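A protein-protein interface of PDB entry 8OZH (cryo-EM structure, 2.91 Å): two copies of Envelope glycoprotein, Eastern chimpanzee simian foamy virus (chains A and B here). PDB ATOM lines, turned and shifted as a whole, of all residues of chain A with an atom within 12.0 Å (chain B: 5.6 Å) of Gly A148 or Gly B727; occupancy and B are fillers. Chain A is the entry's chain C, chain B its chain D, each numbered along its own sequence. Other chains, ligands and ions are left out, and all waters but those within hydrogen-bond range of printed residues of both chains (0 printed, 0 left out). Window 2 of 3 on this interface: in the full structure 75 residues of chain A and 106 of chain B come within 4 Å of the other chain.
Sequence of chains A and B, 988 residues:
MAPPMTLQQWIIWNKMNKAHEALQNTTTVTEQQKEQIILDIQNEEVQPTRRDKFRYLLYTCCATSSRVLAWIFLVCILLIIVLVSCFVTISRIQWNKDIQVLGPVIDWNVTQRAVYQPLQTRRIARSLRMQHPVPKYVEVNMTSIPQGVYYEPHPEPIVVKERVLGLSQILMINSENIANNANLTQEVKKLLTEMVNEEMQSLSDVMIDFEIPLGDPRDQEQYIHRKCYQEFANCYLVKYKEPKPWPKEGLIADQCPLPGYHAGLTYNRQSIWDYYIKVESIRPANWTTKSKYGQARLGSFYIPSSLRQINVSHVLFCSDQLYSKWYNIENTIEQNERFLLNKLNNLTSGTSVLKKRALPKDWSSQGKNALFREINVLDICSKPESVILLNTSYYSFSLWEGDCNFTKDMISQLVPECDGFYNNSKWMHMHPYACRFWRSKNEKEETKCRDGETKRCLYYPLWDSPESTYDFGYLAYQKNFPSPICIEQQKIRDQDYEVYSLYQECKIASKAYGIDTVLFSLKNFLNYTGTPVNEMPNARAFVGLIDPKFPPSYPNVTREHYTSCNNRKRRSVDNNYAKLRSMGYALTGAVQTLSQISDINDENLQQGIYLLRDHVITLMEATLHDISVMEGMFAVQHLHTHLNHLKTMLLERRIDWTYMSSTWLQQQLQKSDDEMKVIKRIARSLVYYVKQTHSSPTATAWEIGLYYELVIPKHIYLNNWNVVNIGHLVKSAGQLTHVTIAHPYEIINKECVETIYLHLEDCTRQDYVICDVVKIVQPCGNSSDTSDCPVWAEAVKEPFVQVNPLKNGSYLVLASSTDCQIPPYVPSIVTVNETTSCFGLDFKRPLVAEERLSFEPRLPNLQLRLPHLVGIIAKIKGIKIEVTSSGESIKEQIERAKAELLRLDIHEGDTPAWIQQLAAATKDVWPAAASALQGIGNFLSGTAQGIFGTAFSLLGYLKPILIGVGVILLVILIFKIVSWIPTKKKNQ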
ATOM      1  N   THR A 143      -3.397  23.472  21.684  1.00  0.00           N
ATOM      2  CA  THR A 143      -3.344  22.067  21.192  1.00  0.00           C
ATOM      3  C   THR A 143      -4.682  21.364  21.422  1.00  0.00           C
ATOM      4  O   THR A 143      -5.483  21.859  22.221  1.00  0.00           O
ATOM      5  CB  THR A 143      -2.193  21.272  21.816  1.00  0.00           C
ATOM      6  OG1 THR A 143      -2.375  21.181  23.229  1.00  0.00           O
ATOM      7  CG2 THR A 143      -0.845  21.886  21.518  1.00  0.00           C
ATOM      8  N   SER A 144      -4.891  20.252  20.721  1.00  0.00           N
ATOM      9  CA  SER A 144      -6.164  19.494  20.650  1.00  0.00           C
ATOM     10  C   SER A 144      -6.202  18.397  21.714  1.00  0.00           C
ATOM     11  O   SER A 144      -5.150  18.072  22.283  1.00  0.00           O
ATOM     12  CB  SER A 144      -6.362  18.905  19.279  1.00  0.00           C
ATOM     13  OG  SER A 144      -6.450  19.928  18.302  1.00  0.00           O
ATOM     14  N   ILE A 145      -7.394  17.845  21.920  1.00  0.00           N
ATOM     15  CA  ILE A 145      -7.747  16.823  22.943  1.00  0.00           C
ATOM     16  C   ILE A 145      -8.582  15.761  22.221  1.00  0.00           C
ATOM     17  O   ILE A 145      -9.815  15.822  22.204  1.00  0.00           O
ATOM     18  CB  ILE A 145      -8.486  17.512  24.113  1.00  0.00           C
ATOM     19  CG1 ILE A 145      -7.598  18.525  24.828  1.00  0.00           C
ATOM     20  CG2 ILE A 145      -9.029  16.531  25.123  1.00  0.00           C
ATOM     21  CD1 ILE A 145      -8.387  19.623  25.499  1.00  0.00           C
ATOM     22  N   PRO A 146      -7.937  14.783  21.544  1.00  0.00           N
ATOM     23  CA  PRO A 146      -8.662  13.744  20.808  1.00  0.00           C
ATOM     24  C   PRO A 146      -9.803  13.106  21.614  1.00  0.00           C
ATOM     25  O   PRO A 146      -9.578  12.741  22.750  1.00  0.00           O
ATOM     26  CB  PRO A 146      -7.574  12.709  20.496  1.00  0.00           C
ATOM     27  CG  PRO A 146      -6.312  13.534  20.412  1.00  0.00           C
ATOM     28  CD  PRO A 146      -6.479  14.633  21.440  1.00  0.00           C
ATOM     29  N   GLN A 147     -11.000  13.062  21.019  1.00  0.00           N
ATOM     30  CA  GLN A 147     -12.261  12.502  21.583  1.00  0.00           C
ATOM     31  C   GLN A 147     -12.781  13.377  22.736  1.00  0.00           C
ATOM     32  O   GLN A 147     -13.830  13.027  23.285  1.00  0.00           O
ATOM     33  CB  GLN A 147     -12.078  11.045  22.035  1.00  0.00           C
ATOM     34  CG  GLN A 147     -11.286  10.181  21.052  1.00  0.00           C
ATOM     35  CD  GLN A 147     -11.609   8.702  21.081  1.00  0.00           C
ATOM     36  OE1 GLN A 147     -12.406   8.231  21.886  1.00  0.00           O
ATOM     37  NE2 GLN A 147     -10.988   7.941  20.195  1.00  0.00           N
ATOM     38  N   GLY A 148     -12.119  14.483  23.079  1.00  0.00           N
ATOM     39  CA  GLY A 148     -12.483  15.298  24.252  1.00  0.00           C
ATOM     40  C   GLY A 148     -12.116  14.636  25.575  1.00  0.00           C
ATOM     41  O   GLY A 148     -12.679  15.056  26.605  1.00  0.00           O
ATOM     42  N   VAL A 149     -11.181  13.682  25.577  1.00  0.00           N
ATOM     43  CA  VAL A 149     -10.692  12.992  26.810  1.00  0.00           C
ATOM     44  C   VAL A 149      -9.413  13.688  27.281  1.00  0.00           C
ATOM     45  O   VAL A 149      -8.464  13.716  26.483  1.00  0.00           O
ATOM     46  CB  VAL A 149     -10.410  11.501  26.543  1.00  0.00           C
ATOM     47  CG1 VAL A 149      -9.818  10.817  27.765  1.00  0.00           C
ATOM     48  CG2 VAL A 149     -11.643  10.758  26.045  1.00  0.00           C
ATOM     49  N   TYR A 150      -9.376  14.180  28.522  1.00  0.00           N
ATOM     50  CA  TYR A 150      -8.143  14.605  29.239  1.00  0.00           C
ATOM     51  C   TYR A 150      -7.890  13.638  30.407  1.00  0.00           C
ATOM     52  O   TYR A 150      -8.772  12.811  30.669  1.00  0.00           O
ATOM     53  CB  TYR A 150      -8.265  16.068  29.682  1.00  0.00           C
ATOM     54  CG  TYR A 150      -6.968  16.683  30.150  1.00  0.00           C
ATOM     55  CD1 TYR A 150      -5.853  16.719  29.322  1.00  0.00           C
ATOM     56  CD2 TYR A 150      -6.836  17.183  31.437  1.00  0.00           C
ATOM     57  CE1 TYR A 150      -4.650  17.257  29.749  1.00  0.00           C
ATOM     58  CE2 TYR A 150      -5.641  17.726  31.881  1.00  0.00           C
ATOM     59  CZ  TYR A 150      -4.547  17.767  31.033  1.00  0.00           C
ATOM     60  OH  TYR A 150      -3.366  18.290  31.477  1.00  0.00           O
ATOM     61  N   TYR A 151      -6.728  13.720  31.068  1.00  0.00           N
ATOM     62  CA  TYR A 151      -6.269  12.752  32.105  1.00  0.00           C
ATOM     63  C   TYR A 151      -5.431  13.442  33.189  1.00  0.00           C
ATOM     64  O   TYR A 151      -4.890  14.533  32.932  1.00  0.00           O
ATOM     65  CB  TYR A 151      -5.464  11.615  31.467  1.00  0.00           C
ATOM     66  CG  TYR A 151      -4.835  11.986  30.154  1.00  0.00           C
ATOM     67  CD1 TYR A 151      -3.661  12.723  30.105  1.00  0.00           C
ATOM     68  CD2 TYR A 151      -5.458  11.667  28.960  1.00  0.00           C
ATOM     69  CE1 TYR A 151      -3.096  13.100  28.895  1.00  0.00           C
ATOM     70  CE2 TYR A 151      -4.913  12.041  27.742  1.00  0.00           C
ATOM     71  CZ  TYR A 151      -3.728  12.762  27.708  1.00  0.00           C
ATOM     72  OH  TYR A 151      -3.195  13.121  26.504  1.00  0.00           O
ATOM     73  N   GLU A 152      -5.347  12.801  34.362  1.00  0.00           N
ATOM     74  CA  GLU A 152      -4.565  13.218  35.557  1.00  0.00           C
ATOM     75  C   GLU A 152      -3.921  11.982  36.180  1.00  0.00           C
ATOM     76  O   GLU A 152      -4.544  10.921  36.188  1.00  0.00           O
ATOM     77  CB  GLU A 152      -5.485  13.845  36.605  1.00  0.00           C
ATOM     78  CG  GLU A 152      -6.159  15.130  36.150  1.00  0.00           C
ATOM     79  CD  GLU A 152      -7.293  15.646  37.032  1.00  0.00           C
ATOM     80  OE1 GLU A 152      -7.625  16.854  36.925  1.00  0.00           O
ATOM     81  OE2 GLU A 152      -7.862  14.841  37.816  1.00  0.00           O
ATOM     82  N   VAL B 724     -10.788  12.042  32.399  1.00  0.00           N
ATOM     83  CA  VAL B 724     -11.614  13.272  32.620  1.00  0.00           C
ATOM     84  C   VAL B 724     -12.334  13.629  31.308  1.00  0.00           C
ATOM     85  O   VAL B 724     -11.681  14.193  30.422  1.00  0.00           O
ATOM     86  CB  VAL B 724     -10.745  14.456  33.095  1.00  0.00           C
ATOM     87  CG1 VAL B 724     -11.554  15.739  33.224  1.00  0.00           C
ATOM     88  CG2 VAL B 724     -10.009  14.155  34.390  1.00  0.00           C
ATOM     89  N   ASN B 725     -13.635  13.353  31.192  1.00  0.00           N
ATOM     90  CA  ASN B 725     -14.435  13.637  29.968  1.00  0.00           C
ATOM     91  C   ASN B 725     -14.686  15.151  29.892  1.00  0.00           C
ATOM     92  O   ASN B 725     -15.147  15.700  30.899  1.00  0.00           O
ATOM     93  CB  ASN B 725     -15.736  12.824  29.965  1.00  0.00           C
ATOM     94  CG  ASN B 725     -16.192  12.338  28.600  1.00  0.00           C
ATOM     95  OD1 ASN B 725     -15.460  12.379  27.610  1.00  0.00           O
ATOM     96  ND2 ASN B 725     -17.417  11.840  28.537  1.00  0.00           N
ATOM     97  N   ILE B 726     -14.359  15.812  28.777  1.00  0.00           N
ATOM     98  CA  ILE B 726     -14.592  17.276  28.579  1.00  0.00           C
ATOM     99  C   ILE B 726     -15.722  17.485  27.561  1.00  0.00           C
ATOM    100  O   ILE B 726     -16.590  18.335  27.828  1.00  0.00           O
ATOM    101  CB  ILE B 726     -13.307  18.017  28.156  1.00  0.00           C
ATOM    102  CG1 ILE B 726     -12.187  17.865  29.191  1.00  0.00           C
ATOM    103  CG2 ILE B 726     -13.602  19.482  27.849  1.00  0.00           C
ATOM    104  CD1 ILE B 726     -12.304  18.778  30.384  1.00  0.00           C
ATOM    105  N   GLY B 727     -15.705  16.783  26.432  1.00  0.00           N
ATOM    106  CA  GLY B 727     -16.778  16.862  25.429  1.00  0.00           C
ATOM    107  C   GLY B 727     -16.554  18.009  24.458  1.00  0.00           C
ATOM    108  O   GLY B 727     -15.391  18.335  24.187  1.00  0.00           O
ATOM    109  N   HIS B 728     -17.637  18.605  23.960  1.00  0.00           N
ATOM    110  CA  HIS B 728     -17.667  19.543  22.810  1.00  0.00           C
ATOM    111  C   HIS B 728     -19.023  20.261  22.804  1.00  0.00           C
ATOM    112  O   HIS B 728     -20.046  19.596  23.112  1.00  0.00           O
ATOM    113  CB  HIS B 728     -17.442  18.733  21.531  1.00  0.00           C
ATOM    114  CG  HIS B 728     -16.904  19.489  20.360  1.00  0.00           C
ATOM    115  ND1 HIS B 728     -17.559  20.570  19.807  1.00  0.00           N
ATOM    116  CD2 HIS B 728     -15.805  19.278  19.597  1.00  0.00           C
ATOM    117  CE1 HIS B 728     -16.869  21.012  18.773  1.00  0.00           C
ATOM    118  NE2 HIS B 728     -15.785  20.238  18.623  1.00  0.00           N
ATOM    119  N   LEU B 729     -19.055  21.550  22.463  1.00  0.00           N
ATOM    120  CA  LEU B 729     -20.317  22.324  22.303  1.00  0.00           C
ATOM    121  C   LEU B 729     -20.757  22.279  20.834  1.00  0.00           C
ATOM    122  O   LEU B 729     -19.881  22.261  19.947  1.00  0.00           O
ATOM    123  CB  LEU B 729     -20.101  23.764  22.771  1.00  0.00           C
ATOM    124  CG  LEU B 729     -19.755  23.940  24.247  1.00  0.00           C
ATOM    125  CD1 LEU B 729     -19.376  25.384  24.546  1.00  0.00           C
ATOM    126  CD2 LEU B 729     -20.909  23.510  25.130  1.00  0.00           C
ATOM    127  N   HIS B 738     -24.334  20.624  24.804  1.00  0.00           N
ATOM    128  CA  HIS B 738     -23.057  19.991  25.222  1.00  0.00           C
ATOM    129  C   HIS B 738     -23.111  18.503  24.867  1.00  0.00           C
ATOM    130  O   HIS B 738     -24.082  17.850  25.295  1.00  0.00           O
ATOM    131  CB  HIS B 738     -22.798  20.263  26.700  1.00  0.00           C
ATOM    132  CG  HIS B 738     -21.469  19.787  27.170  1.00  0.00           C
ATOM    133  ND1 HIS B 738     -21.151  19.699  28.504  1.00  0.00           N
ATOM    134  CD2 HIS B 738     -20.377  19.373  26.496  1.00  0.00           C
ATOM    135  CE1 HIS B 738     -19.916  19.251  28.628  1.00  0.00           C
ATOM    136  NE2 HIS B 738     -19.420  19.044  27.412  1.00  0.00           N
ATOM    137  N   VAL B 739     -22.136  18.002  24.091  1.00  0.00           N
ATOM    138  CA  VAL B 739     -22.114  16.598  23.575  1.00  0.00           C
ATOM    139  C   VAL B 739     -20.950  15.842  24.221  1.00  0.00           C
ATOM    140  O   VAL B 739     -19.851  16.403  24.265  1.00  0.00           O
ATOM    141  CB  VAL B 739     -22.038  16.561  22.035  1.00  0.00           C
ATOM    142  CG1 VAL B 739     -21.780  15.160  21.506  1.00  0.00           C
ATOM    143  CG2 VAL B 739     -23.299  17.120  21.393  1.00  0.00           C
ATOM    144  N   THR B 740     -21.184  14.605  24.673  1.00  0.00           N
ATOM    145  CA  THR B 740     -20.154  13.764  25.353  1.00  0.00           C
ATOM    146  C   THR B 740     -20.222  12.306  24.897  1.00  0.00           C
ATOM    147  O   THR B 740     -21.344  11.803  24.672  1.00  0.00           O
ATOM    148  CB  THR B 740     -20.315  13.788  26.874  1.00  0.00           C
ATOM    149  OG1 THR B 740     -21.715  13.817  27.146  1.00  0.00           O
ATOM    150  CG2 THR B 740     -19.663  14.983  27.526  1.00  0.00           C
ATOM    151  N   HIS B 743     -17.246   6.552  27.488  1.00  0.00           N
ATOM    152  CA  HIS B 743     -16.055   5.684  27.278  1.00  0.00           C
ATOM    153  C   HIS B 743     -16.219   4.409  28.098  1.00  0.00           C
ATOM    154  O   HIS B 743     -16.678   4.467  29.235  1.00  0.00           O
ATOM    155  CB  HIS B 743     -14.769   6.453  27.603  1.00  0.00           C
ATOM    156  CG  HIS B 743     -14.665   7.716  26.817  1.00  0.00           C
ATOM    157  ND1 HIS B 743     -14.241   7.732  25.493  1.00  0.00           N
ATOM    158  CD2 HIS B 743     -14.996   8.989  27.131  1.00  0.00           C
ATOM    159  CE1 HIS B 743     -14.286   8.969  25.038  1.00  0.00           C
ATOM    160  NE2 HIS B 743     -14.758   9.761  26.023  1.00  0.00           N
ATOM    161  N   LEU B 814     -13.120  25.637  27.500  1.00  0.00           N
ATOM    162  CA  LEU B 814     -14.302  25.371  26.638  1.00  0.00           C
ATOM    163  C   LEU B 814     -15.289  26.537  26.809  1.00  0.00           C
ATOM    164  O   LEU B 814     -15.665  26.814  27.961  1.00  0.00           O
ATOM    165  CB  LEU B 814     -14.910  24.020  27.036  1.00  0.00           C
ATOM    166  CG  LEU B 814     -16.125  23.571  26.222  1.00  0.00           C
ATOM    167  CD1 LEU B 814     -15.772  23.358  24.755  1.00  0.00           C
ATOM    168  CD2 LEU B 814     -16.720  22.294  26.794  1.00  0.00           C
ATOM    169  N   PRO B 827     -12.826  22.390  22.466  1.00  0.00           N
ATOM    170  CA  PRO B 827     -11.940  22.631  23.614  1.00  0.00           C
ATOM    171  C   PRO B 827     -10.452  22.655  23.233  1.00  0.00           C
ATOM    172  O   PRO B 827     -10.125  22.113  22.196  1.00  0.00           O
ATOM    173  CB  PRO B 827     -12.213  21.445  24.549  1.00  0.00           C
ATOM    174  CG  PRO B 827     -12.641  20.343  23.609  1.00  0.00           C
ATOM    175  CD  PRO B 827     -13.370  21.025  22.465  1.00  0.00           C
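N of Ile B726 lies within hydrogen-bond range of O of Gly A148, at 2.8 Å. The backbone carbonyl oxygen (O) of Tyr A150 lies within hydrogen-bond range of the backbone NH (N) of Val B724, 2.8 Å away. The backbone NH (N) of Gly B727 sits at hydrogen-bond distance from the backbone carbonyl oxygen (O) of Gly A148.
A ring nitrogen (NE2) of His B743 is in hydrogen-bond range of the side-chain amide oxygen (OD1) of Asn B725. O of Ile B726 is in hydrogen-bond range of NE2 of His B738, at 2.9 Å.
Among the printed residues, merely in contact across the chains: Gln A147 with His B743, Gly A148 with Asn B725, Val A149 with Val B724 and Val A149 with His B743.
Printed residues of chain B within 4 Å of Gln A147: His B743. Of chain B, only Asn B725 (3.9 Å), Ile B726 (2.8 Å) and Gly B727 (3.5 Å) come within 4 Å of Gly A148. Of the printed residues of chain B, Val A149 touches Val B724 (3.9 Å) and His B743 (3.3 Å). Printed residues of chain B within 4 Å of Tyr A150: Val B724 (2.8 Å). Printed residues of chain A within 4 Å of Val B724: Val A149 (3.9 Å) and Tyr A150 (2.8 Å). Ile B726 touches one residue of chain A. Of chain A, only Gly A148 (3.5 Å) comes within 4 Å of Gly B727. No residue of chain A comes within 4 Å of Leu B729. His B738 touches none of the printed residues of chain A. No residue of chain A comes within 4 Å of Thr B740. Of the printed residues of chain A, His B743 touches Gln A147 (3.7 Å) and Val A149 (3.3 Å). No residue of chain A comes within 4 Å of Pro B827. The nearest residue of chain A that does not touch Gly B727 is Gln A147 (5.2 Å).
Printed residues of chain A that touch a printed residue of chain B: Gln A147, Gly A148, Val A149 and Tyr A150. Hydrophobic or aromatic side chains of chain A that line the printed part of chain B: Val A149 and Tyr A150. Among the printed residues, 7 pairs touch across the chains. Among the printed residues, no Asp or Glu carboxylate lies within 4 Å of a Lys or Arg side-chain nitrogen of the other chain.
No position is printed for both chains.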
